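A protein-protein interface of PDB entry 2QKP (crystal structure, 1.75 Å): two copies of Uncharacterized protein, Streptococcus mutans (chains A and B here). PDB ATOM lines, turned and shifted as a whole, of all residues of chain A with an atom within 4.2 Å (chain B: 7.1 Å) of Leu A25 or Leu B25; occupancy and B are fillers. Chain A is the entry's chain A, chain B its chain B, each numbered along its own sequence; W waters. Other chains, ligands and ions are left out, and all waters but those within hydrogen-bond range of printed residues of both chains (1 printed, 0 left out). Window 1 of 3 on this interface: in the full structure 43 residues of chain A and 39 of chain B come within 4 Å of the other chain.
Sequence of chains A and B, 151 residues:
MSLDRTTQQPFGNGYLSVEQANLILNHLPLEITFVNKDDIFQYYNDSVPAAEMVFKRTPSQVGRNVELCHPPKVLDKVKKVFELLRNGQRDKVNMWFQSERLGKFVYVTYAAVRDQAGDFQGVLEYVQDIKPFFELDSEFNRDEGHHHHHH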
ATOM      1  N   ALA A  21     -19.379   7.761  -4.741  1.00  0.00           N
ATOM      2  CA  ALA A  21     -20.793   8.108  -5.037  1.00  0.00           C
ATOM      3  C   ALA A  21     -20.799   8.963  -6.302  1.00  0.00           C
ATOM      4  O   ALA A  21     -21.632   8.768  -7.182  1.00  0.00           O
ATOM      5  CB  ALA A  21     -21.462   8.822  -3.884  1.00  0.00           C
ATOM      6  N   ASN A  22     -19.874   9.914  -6.392  1.00  0.00           N
ATOM      7  CA  ASN A  22     -19.744  10.731  -7.601  1.00  0.00           C
ATOM      8  C   ASN A  22     -19.436   9.887  -8.839  1.00  0.00           C
ATOM      9  O   ASN A  22     -20.064  10.078  -9.886  1.00  0.00           O
ATOM     10  CB  ASN A  22     -18.662  11.836  -7.409  1.00  0.00           C
ATOM     11  CG  ASN A  22     -18.625  12.804  -8.586  1.00  0.00           C
ATOM     12  OD1 ASN A  22     -19.641  13.384  -8.921  1.00  0.00           O
ATOM     13  ND2 ASN A  22     -17.454  12.951  -9.237  1.00  0.00           N
ATOM     14  N   LEU A  23     -18.479   8.950  -8.744  1.00  0.00           N
ATOM     15  CA  LEU A  23     -18.210   8.058  -9.886  1.00  0.00           C
ATOM     16  C   LEU A  23     -19.463   7.281 -10.310  1.00  0.00           C
ATOM     17  O   LEU A  23     -19.760   7.143 -11.486  1.00  0.00           O
ATOM     18  CB  LEU A  23     -17.146   7.039  -9.516  1.00  0.00           C
ATOM     19  CG  LEU A  23     -15.718   7.582  -9.539  1.00  0.00           C
ATOM     20  CD1 LEU A  23     -14.843   6.611  -8.787  1.00  0.00           C
ATOM     21  CD2 LEU A  23     -15.207   7.815 -10.980  1.00  0.00           C
ATOM     22  N   ILE A  24     -20.204   6.793  -9.327  1.00  0.00           N
ATOM     23  CA  ILE A  24     -21.430   6.018  -9.650  1.00  0.00           C
ATOM     24  C   ILE A  24     -22.427   6.883 -10.407  1.00  0.00           C
ATOM     25  O   ILE A  24     -22.938   6.487 -11.438  1.00  0.00           O
ATOM     26  CB  ILE A  24     -22.041   5.417  -8.389  1.00  0.00           C
ATOM     27  CG1 ILE A  24     -21.165   4.239  -7.908  1.00  0.00           C
ATOM     28  CG2 ILE A  24     -23.501   4.959  -8.663  1.00  0.00           C
ATOM     29  CD1 ILE A  24     -21.424   3.859  -6.436  1.00  0.00           C
ATOM     30  N   LEU A  25     -22.672   8.093  -9.913  1.00  0.00           N
ATOM     31  CA  LEU A  25     -23.636   8.993 -10.554  1.00  0.00           C
ATOM     32  C   LEU A  25     -23.236   9.296 -11.975  1.00  0.00           C
ATOM     33  O   LEU A  25     -24.097   9.480 -12.848  1.00  0.00           O
ATOM     34  CB  LEU A  25     -23.804  10.285  -9.751  1.00  0.00           C
ATOM     35  CG  LEU A  25     -24.622  10.135  -8.462  1.00  0.00           C
ATOM     36  CD1 LEU A  25     -24.374  11.314  -7.512  1.00  0.00           C
ATOM     37  CD2 LEU A  25     -26.143   9.925  -8.696  1.00  0.00           C
ATOM     38  N   ASN A  26     -21.923   9.367 -12.212  1.00  0.00           N
ATOM     39  CA  ASN A  26     -21.406   9.618 -13.579  1.00  0.00           C
ATOM     40  C   ASN A  26     -21.386   8.406 -14.518  1.00  0.00           C
ATOM     41  O   ASN A  26     -21.260   8.587 -15.742  1.00  0.00           O
ATOM     42  CB  ASN A  26     -20.001  10.211 -13.480  1.00  0.00           C
ATOM     43  CG  ASN A  26     -20.006  11.624 -12.885  1.00  0.00           C
ATOM     44  OD1 ASN A  26     -21.045  12.289 -12.860  1.00  0.00           O
ATOM     45  ND2 ASN A  26     -18.845  12.080 -12.390  1.00  0.00           N
ATOM     46  N   HIS A  27     -21.483   7.199 -13.962  1.00  0.00           N
ATOM     47  CA  HIS A  27     -21.460   5.960 -14.776  1.00  0.00           C
ATOM     48  C   HIS A  27     -22.837   5.388 -15.039  1.00  0.00           C
ATOM     49  O   HIS A  27     -22.985   4.389 -15.765  1.00  0.00           O
ATOM     50  CB  HIS A  27     -20.557   4.888 -14.149  1.00  0.00           C
ATOM     51  CG  HIS A  27     -19.100   5.135 -14.379  1.00  0.00           C
ATOM     52  ND1 HIS A  27     -18.390   6.069 -13.658  1.00  0.00           N
ATOM     53  CD2 HIS A  27     -18.226   4.589 -15.265  1.00  0.00           C
ATOM     54  CE1 HIS A  27     -17.129   6.071 -14.073  1.00  0.00           C
ATOM     55  NE2 HIS A  27     -17.007   5.193 -15.056  1.00  0.00           N
ATOM     56  N   LEU A  28     -23.868   6.005 -14.472  1.00  0.00           N
ATOM     57  CA  LEU A  28     -25.227   5.547 -14.761  1.00  0.00           C
ATOM     58  C   LEU A  28     -25.630   5.999 -16.157  1.00  0.00           C
ATOM     59  O   LEU A  28     -25.170   7.046 -16.608  1.00  0.00           O
ATOM     60  CB  LEU A  28     -26.193   6.053 -13.693  1.00  0.00           C
ATOM     61  CG  LEU A  28     -26.028   5.420 -12.294  1.00  0.00           C
ATOM     62  CD1 LEU A  28     -26.808   6.249 -11.269  1.00  0.00           C
ATOM     63  CD2 LEU A  28     -26.503   3.962 -12.261  1.00  0.00           C
ATOM     64  N   TYR A  43     -27.250  20.879  -9.623  1.00  0.00           N
ATOM     65  CA  TYR A  43     -26.406  19.738  -9.982  1.00  0.00           C
ATOM     66  C   TYR A  43     -26.842  19.054 -11.263  1.00  0.00           C
ATOM     67  O   TYR A  43     -28.044  18.867 -11.483  1.00  0.00           O
ATOM     68  CB  TYR A  43     -26.480  18.718  -8.832  1.00  0.00           C
ATOM     69  CG  TYR A  43     -25.994  17.323  -9.212  1.00  0.00           C
ATOM     70  CD1 TYR A  43     -24.622  17.010  -9.190  1.00  0.00           C
ATOM     71  CD2 TYR A  43     -26.896  16.323  -9.593  1.00  0.00           C
ATOM     72  CE1 TYR A  43     -24.148  15.721  -9.523  1.00  0.00           C
ATOM     73  CE2 TYR A  43     -26.436  15.041  -9.952  1.00  0.00           C
ATOM     74  CZ  TYR A  43     -25.062  14.757  -9.925  1.00  0.00           C
ATOM     75  OH  TYR A  43     -24.651  13.498 -10.241  1.00  0.00           O
ATOM     76  N   ASN A  45     -25.141  15.524 -13.606  1.00  0.00           N
ATOM     77  CA  ASN A  45     -24.033  14.566 -13.578  1.00  0.00           C
ATOM     78  C   ASN A  45     -23.116  14.780 -14.790  1.00  0.00           C
ATOM     79  O   ASN A  45     -23.431  15.565 -15.682  1.00  0.00           O
ATOM     80  CB  ASN A  45     -24.526  13.101 -13.440  1.00  0.00           C
ATOM     81  CG  ASN A  45     -25.308  12.612 -14.615  1.00  0.00           C
ATOM     82  OD1 ASN A  45     -25.874  13.380 -15.409  1.00  0.00           O
ATOM     83  ND2 ASN A  45     -25.369  11.279 -14.736  1.00  0.00           N
ATOM     84  N   PHE B  11     -19.989  17.694  -6.897  1.00  0.00           N
ATOM     85  CA  PHE B  11     -20.431  16.421  -7.467  1.00  0.00           C
ATOM     86  C   PHE B  11     -20.714  16.737  -8.927  1.00  0.00           C
ATOM     87  O   PHE B  11     -21.420  17.692  -9.200  1.00  0.00           O
ATOM     88  CB  PHE B  11     -21.751  15.990  -6.819  1.00  0.00           C
ATOM     89  CG  PHE B  11     -21.609  15.081  -5.627  1.00  0.00           C
ATOM     90  CD1 PHE B  11     -21.676  13.700  -5.782  1.00  0.00           C
ATOM     91  CD2 PHE B  11     -21.494  15.603  -4.360  1.00  0.00           C
ATOM     92  CE1 PHE B  11     -21.582  12.840  -4.656  1.00  0.00           C
ATOM     93  CE2 PHE B  11     -21.434  14.770  -3.242  1.00  0.00           C
ATOM     94  CZ  PHE B  11     -21.456  13.375  -3.415  1.00  0.00           C
ATOM     95  N   GLY B  12     -20.220  15.922  -9.859  1.00  0.00           N
ATOM     96  CA  GLY B  12     -20.523  16.138 -11.278  1.00  0.00           C
ATOM     97  C   GLY B  12     -20.244  17.555 -11.735  1.00  0.00           C
ATOM     98  O   GLY B  12     -19.160  18.100 -11.479  1.00  0.00           O
ATOM     99  N   LEU B  16     -23.698  18.843  -4.463  1.00  0.00           N
ATOM    100  CA  LEU B  16     -24.694  18.120  -3.682  1.00  0.00           C
ATOM    101  C   LEU B  16     -24.101  17.911  -2.321  1.00  0.00           C
ATOM    102  O   LEU B  16     -22.868  17.814  -2.167  1.00  0.00           O
ATOM    103  CB  LEU B  16     -25.000  16.726  -4.252  1.00  0.00           C
ATOM    104  CG  LEU B  16     -25.613  16.563  -5.644  1.00  0.00           C
ATOM    105  CD1 LEU B  16     -25.541  15.102  -6.084  1.00  0.00           C
ATOM    106  CD2 LEU B  16     -27.076  17.004  -5.639  1.00  0.00           C
ATOM    107  N   GLN B  20     -28.209  14.711  -0.030  1.00  0.00           N
ATOM    108  CA  GLN B  20     -28.890  14.785  -1.322  1.00  0.00           C
ATOM    109  C   GLN B  20     -28.412  13.705  -2.287  1.00  0.00           C
ATOM    110  O   GLN B  20     -29.239  13.088  -2.990  1.00  0.00           O
ATOM    111  CB  GLN B  20     -28.725  16.155  -1.947  1.00  0.00           C
ATOM    112  CG  GLN B  20     -29.385  17.269  -1.117  1.00  0.00           C
ATOM    113  CD  GLN B  20     -28.968  18.625  -1.571  1.00  0.00           C
ATOM    114  OE1 GLN B  20     -27.814  18.836  -1.944  1.00  0.00           O
ATOM    115  NE2 GLN B  20     -29.911  19.575  -1.550  1.00  0.00           N
ATOM    116  N   ALA B  21     -27.102  13.478  -2.338  1.00  0.00           N
ATOM    117  CA  ALA B  21     -26.563  12.427  -3.232  1.00  0.00           C
ATOM    118  C   ALA B  21     -27.188  11.081  -2.857  1.00  0.00           C
ATOM    119  O   ALA B  21     -27.583  10.302  -3.728  1.00  0.00           O
ATOM    120  CB  ALA B  21     -25.034  12.375  -3.126  1.00  0.00           C
ATOM    121  N   ASN B  22     -27.300  10.797  -1.562  1.00  0.00           N
ATOM    122  CA  ASN B  22     -27.893   9.550  -1.116  1.00  0.00           C
ATOM    123  C   ASN B  22     -29.371   9.453  -1.526  1.00  0.00           C
ATOM    124  O   ASN B  22     -29.847   8.387  -1.969  1.00  0.00           O
ATOM    125  CB  ASN B  22     -27.750   9.429   0.406  1.00  0.00           C
ATOM    126  CG  ASN B  22     -28.229   8.101   0.945  1.00  0.00           C
ATOM    127  OD1 ASN B  22     -27.763   7.033   0.522  1.00  0.00           O
ATOM    128  ND2 ASN B  22     -29.177   8.150   1.889  1.00  0.00           N
ATOM    129  N   LEU B  23     -30.118  10.527  -1.279  1.00  0.00           N
ATOM    130  CA  LEU B  23     -31.535  10.566  -1.728  1.00  0.00           C
ATOM    131  C   LEU B  23     -31.644  10.282  -3.222  1.00  0.00           C
ATOM    132  O   LEU B  23     -32.547   9.542  -3.682  1.00  0.00           O
ATOM    133  CB  LEU B  23     -32.114  11.946  -1.412  1.00  0.00           C
ATOM    134  CG  LEU B  23     -32.408  12.115   0.085  1.00  0.00           C
ATOM    135  CD1 LEU B  23     -32.697  13.604   0.387  1.00  0.00           C
ATOM    136  CD2 LEU B  23     -33.536  11.217   0.575  1.00  0.00           C
ATOM    137  N   ILE B  24     -30.761  10.898  -4.006  1.00  0.00           N
ATOM    138  CA  ILE B  24     -30.810  10.716  -5.449  1.00  0.00           C
ATOM    139  C   ILE B  24     -30.637   9.235  -5.802  1.00  0.00           C
ATOM    140  O   ILE B  24     -31.455   8.651  -6.555  1.00  0.00           O
ATOM    141  CB  ILE B  24     -29.777  11.626  -6.171  1.00  0.00           C
ATOM    142  CG1 ILE B  24     -30.284  13.104  -6.056  1.00  0.00           C
ATOM    143  CG2 ILE B  24     -29.660  11.204  -7.655  1.00  0.00           C
ATOM    144  CD1 ILE B  24     -29.268  14.160  -6.578  1.00  0.00           C
ATOM    145  N   LEU B  25     -29.592   8.626  -5.244  1.00  0.00           N
ATOM    146  CA  LEU B  25     -29.340   7.184  -5.506  1.00  0.00           C
ATOM    147  C   LEU B  25     -30.548   6.307  -5.125  1.00  0.00           C
ATOM    148  O   LEU B  25     -30.847   5.303  -5.813  1.00  0.00           O
ATOM    149  CB  LEU B  25     -28.042   6.728  -4.806  1.00  0.00           C
ATOM    150  CG  LEU B  25     -26.782   7.350  -5.467  1.00  0.00           C
ATOM    151  CD1 LEU B  25     -25.525   7.247  -4.543  1.00  0.00           C
ATOM    152  CD2 LEU B  25     -26.505   6.658  -6.785  1.00  0.00           C
ATOM    153  N   ASN B  26     -31.211   6.679  -4.032  1.00  0.00           N
ATOM    154  CA  ASN B  26     -32.395   5.986  -3.530  1.00  0.00           C
ATOM    155  C   ASN B  26     -33.704   6.335  -4.259  1.00  0.00           C
ATOM    156  O   ASN B  26     -34.757   5.766  -3.918  1.00  0.00           O
ATOM    157  CB  ASN B  26     -32.574   6.250  -2.029  1.00  0.00           C
ATOM    158  CG  ASN B  26     -31.457   5.625  -1.199  1.00  0.00           C
ATOM    159  OD1 ASN B  26     -30.730   4.776  -1.703  1.00  0.00           O
ATOM    160  ND2 ASN B  26     -31.277   6.095   0.038  1.00  0.00           N
ATOM    161  N   HIS B  27     -33.663   7.275  -5.195  1.00  0.00           N
ATOM    162  CA  HIS B  27     -34.866   7.576  -5.982  1.00  0.00           C
ATOM    163  C   HIS B  27     -34.734   7.220  -7.446  1.00  0.00           C
ATOM    164  O   HIS B  27     -35.595   7.597  -8.241  1.00  0.00           O
ATOM    165  CB  HIS B  27     -35.283   9.047  -5.865  1.00  0.00           C
ATOM    166  CG  HIS B  27     -35.951   9.369  -4.568  1.00  0.00           C
ATOM    167  ND1 HIS B  27     -35.274   9.399  -3.375  1.00  0.00           N
ATOM    168  CD2 HIS B  27     -37.245   9.648  -4.278  1.00  0.00           C
ATOM    169  CE1 HIS B  27     -36.115   9.698  -2.399  1.00  0.00           C
ATOM    170  NE2 HIS B  27     -37.315   9.875  -2.925  1.00  0.00           N
ATOM    171  N   LEU B  28     -33.661   6.550  -7.834  1.00  0.00           N
ATOM    172  CA  LEU B  28     -33.536   6.109  -9.215  1.00  0.00           C
ATOM    173  C   LEU B  28     -34.213   4.738  -9.327  1.00  0.00           C
ATOM    174  O   LEU B  28     -34.192   3.954  -8.378  1.00  0.00           O
ATOM    175  CB  LEU B  28     -32.059   6.045  -9.630  1.00  0.00           C
ATOM    176  CG  LEU B  28     -31.352   7.416  -9.698  1.00  0.00           C
ATOM    177  CD1 LEU B  28     -29.895   7.168  -9.828  1.00  0.00           C
ATOM    178  CD2 LEU B  28     -31.844   8.252 -10.887  1.00  0.00           C
ATOM    179  N   PRO B  29     -34.805   4.429 -10.495  1.00  0.00           N
ATOM    180  CA  PRO B  29     -35.601   3.206 -10.644  1.00  0.00           C
ATOM    181  C   PRO B  29     -34.719   1.989 -10.939  1.00  0.00           C
ATOM    182  O   PRO B  29     -34.930   1.275 -11.943  1.00  0.00           O
ATOM    183  CB  PRO B  29     -36.487   3.534 -11.856  1.00  0.00           C
ATOM    184  CG  PRO B  29     -35.667   4.383 -12.675  1.00  0.00           C
ATOM    185  CD  PRO B  29     -34.797   5.229 -11.737  1.00  0.00           C
ATOM    186  N   LEU B  30     -33.715   1.768 -10.082  1.00  0.00           N
ATOM    187  CA  LEU B  30     -32.696   0.760 -10.366  1.00  0.00           C
ATOM    188  C   LEU B  30     -32.297   0.114  -9.071  1.00  0.00           C
ATOM    189  O   LEU B  30     -32.323   0.762  -8.004  1.00  0.00           O
ATOM    190  CB  LEU B  30     -31.452   1.390 -10.991  1.00  0.00           C
ATOM    191  CG  LEU B  30     -31.605   2.160 -12.307  1.00  0.00           C
ATOM    192  CD1 LEU B  30     -30.394   3.034 -12.546  1.00  0.00           C
ATOM    193  CD2 LEU B  30     -31.802   1.232 -13.487  1.00  0.00           C
ATOM    194  N   ILE B  32     -29.166  -0.833  -7.523  1.00  0.00           N
ATOM    195  CA  ILE B  32     -27.767  -0.454  -7.746  1.00  0.00           C
ATOM    196  C   ILE B  32     -26.893  -1.168  -6.720  1.00  0.00           C
ATOM    197  O   ILE B  32     -27.201  -1.158  -5.527  1.00  0.00           O
ATOM    198  CB  ILE B  32     -27.577   1.063  -7.596  1.00  0.00           C
ATOM    199  CG1 ILE B  32     -28.495   1.817  -8.566  1.00  0.00           C
ATOM    200  CG2 ILE B  32     -26.093   1.458  -7.864  1.00  0.00           C
ATOM    201  CD1 ILE B  32     -28.418   3.402  -8.488  1.00  0.00           C
ATOM    202  N   TYR B  43     -21.886  -1.759  -1.209  1.00  0.00           N
ATOM    203  CA  TYR B  43     -23.027  -0.833  -1.234  1.00  0.00           C
ATOM    204  C   TYR B  43     -24.126  -1.371  -2.119  1.00  0.00           C
ATOM    205  O   TYR B  43     -23.870  -1.889  -3.213  1.00  0.00           O
ATOM    206  CB  TYR B  43     -22.527   0.503  -1.795  1.00  0.00           C
ATOM    207  CG  TYR B  43     -23.636   1.429  -2.289  1.00  0.00           C
ATOM    208  CD1 TYR B  43     -24.340   2.209  -1.385  1.00  0.00           C
ATOM    209  CD2 TYR B  43     -23.966   1.485  -3.653  1.00  0.00           C
ATOM    210  CE1 TYR B  43     -25.387   3.069  -1.816  1.00  0.00           C
ATOM    211  CE2 TYR B  43     -25.019   2.345  -4.101  1.00  0.00           C
ATOM    212  CZ  TYR B  43     -25.694   3.124  -3.166  1.00  0.00           C
ATOM    213  OH  TYR B  43     -26.743   3.967  -3.549  1.00  0.00           O
ATOM    214  N   ASN B  45     -28.239   0.422  -3.139  1.00  0.00           N
ATOM    215  CA  ASN B  45     -29.158   1.523  -2.820  1.00  0.00           C
ATOM    216  C   ASN B  45     -30.430   1.021  -2.138  1.00  0.00           C
ATOM    217  O   ASN B  45     -30.604  -0.184  -1.930  1.00  0.00           O
ATOM    218  CB  ASN B  45     -29.459   2.391  -4.061  1.00  0.00           C
ATOM    219  CG  ASN B  45     -30.229   1.660  -5.136  1.00  0.00           C
ATOM    220  OD1 ASN B  45     -30.248   0.429  -5.183  1.00  0.00           O
ATOM    221  ND2 ASN B  45     -30.872   2.425  -6.014  1.00  0.00           N
ATOM    222  N   ASP B  46     -31.317   1.956  -1.810  1.00  0.00           N
ATOM    223  CA  ASP B  46     -32.545   1.663  -1.098  1.00  0.00           C
ATOM    224  C   ASP B  46     -33.676   2.325  -1.894  1.00  0.00           C
ATOM    225  O   ASP B  46     -34.204   3.347  -1.483  1.00  0.00           O
ATOM    226  CB  ASP B  46     -32.459   2.313   0.288  1.00  0.00           C
ATOM    227  CG  ASP B  46     -33.696   2.040   1.148  1.00  0.00           C
ATOM    228  OD1 ASP B  46     -34.416   1.066   0.862  1.00  0.00           O
ATOM    229  OD2 ASP B  46     -33.932   2.823   2.090  1.00  0.00           O
ATOM    230  N   SER B  47     -34.008   1.769  -3.051  1.00  0.00           N
ATOM    231  CA  SER B  47     -35.012   2.366  -3.913  1.00  0.00           C
ATOM    232  C   SER B  47     -36.166   1.406  -4.092  1.00  0.00           C
ATOM    233  O   SER B  47     -37.315   1.762  -3.857  1.00  0.00           O
ATOM    234  CB  SER B  47     -34.408   2.704  -5.281  1.00  0.00           C
ATOM    235  OG  SER B  47     -35.367   3.378  -6.072  1.00  0.00           O
ATOM    236  N   LEU B 124     -19.842  -1.445 -11.073  1.00  0.00           N
ATOM    237  CA  LEU B 124     -21.194  -0.977 -10.767  1.00  0.00           C
ATOM    238  C   LEU B 124     -22.178  -1.893 -11.481  1.00  0.00           C
ATOM    239  O   LEU B 124     -22.126  -2.047 -12.717  1.00  0.00           O
ATOM    240  CB  LEU B 124     -21.349   0.455 -11.304  1.00  0.00           C
ATOM    241  CG  LEU B 124     -22.727   1.131 -11.253  1.00  0.00           C
ATOM    242  CD1 LEU B 124     -23.130   1.223  -9.794  1.00  0.00           C
ATOM    243  CD2 LEU B 124     -22.658   2.510 -11.885  1.00  0.00           C
HETATM  244  O   HOH W   1     -21.975  13.288 -10.461  1.00  0.00           O
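N of Gly B12 lies within hydrogen-bond range of OD1 of Asn A22 (2.8 Å).
The backbone carbonyl oxygen (O) of Asn A22 lies close to the side-chain amide nitrogen (ND2) of Asn A26 (3.4 Å). The backbone carbonyl oxygen of Leu A23 is in hydrogen-bond range of a ring nitrogen (ND1) of His A27. ND2 of Asn A45 lies within hydrogen-bond range of O of Leu A25, at 2.9 Å. The side-chain amide nitrogen (ND2) of Asn B45 lies within hydrogen-bond range of the backbone carbonyl oxygen (O) of Leu B25 (2.9 Å). OG of Ser B47 is in hydrogen-bond range of O of Leu B28 (2.7 Å).
OD1 of Asn A22 touches CA of Phe B11, 3.5 Å away. Leu B25 touches Ile A24 (CD2 to CG2, 3.9 Å). CD1 of Leu A25 touches CD1 of Phe B11, 3.996 Å away. Ile B24 touches Leu A25 (CG2 to CD2, 3.9 Å). Leu A25 touches Leu B25. CD2 of Leu B124 touches CB of His A27, at 3.9 Å. CD1 of Leu A28 touches CD1 of Leu B28 (3.5 Å). CD1 of Tyr A43 touches O of Phe B11, at 3.3 Å. CE1 of Tyr A43 touches N of Gly B12, 3.9 Å away. Leu B16 touches Tyr A43.
Printed residues of chain B within 4 Å of Leu A25: Phe B11 (3.996 Å), Ile B24 (3.9 Å) and Leu B25 (3.8 Å). Printed residues of chain B within 4 Å of Leu A28: Leu B28. Of the printed residues of chain A, Leu B16 touches Tyr A43 (3.7 Å). Leu B25 touches two residues of chain A. Printed residues of chain A within 4 Å of Leu B28: Leu A28. Ile B32 touches none of the printed residues of chain A. The nearest printed residue of chain A that does not touch Leu B25 is Ala A21 (4.4 Å).
Printed residues of chain A that touch a printed residue of chain B: Asn A22, Ile A24, Leu A25, His A27, Leu A28 and Tyr A43. Hydrophobic or aromatic side chains of chain A that line the printed part of chain B: Ile A24, Leu A25, His A27, Leu A28 and Tyr A43. Along chain A the printed residues that touch a printed residue of chain B span positions 22 to 43. Of the 20 printed residues of chain B, 7 touch a printed residue of chain A. Printed residues of chain B that touch a printed residue of chain A: Phe B11, Gly B12, Leu B16, Ile B24, Leu B25, Leu B28 and Leu B124. Along chain B the printed residues that touch a printed residue of chain A span positions 11 to 124. Among the printed residues, no Asp or Glu carboxylate lies within 4 Å of a Lys or Arg side-chain nitrogen of the other chain.
Ile A24 touches Leu B25, and with the chains exchanged Leu A25 touches Ile B24. Leu B25 touches its own counterpart, Leu A25. Leu B28 touches its own counterpart, Leu A28.
Water W1 lies within hydrogen-bond range of the side-chain hydroxyl of Tyr A43 (2.7 Å), the side-chain amide oxygen of Asn A26 (2.8 Å), the side-chain amide oxygen of Asn A22 (2.8 Å) and the backbone NH of Gly B12 (3.2 Å).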
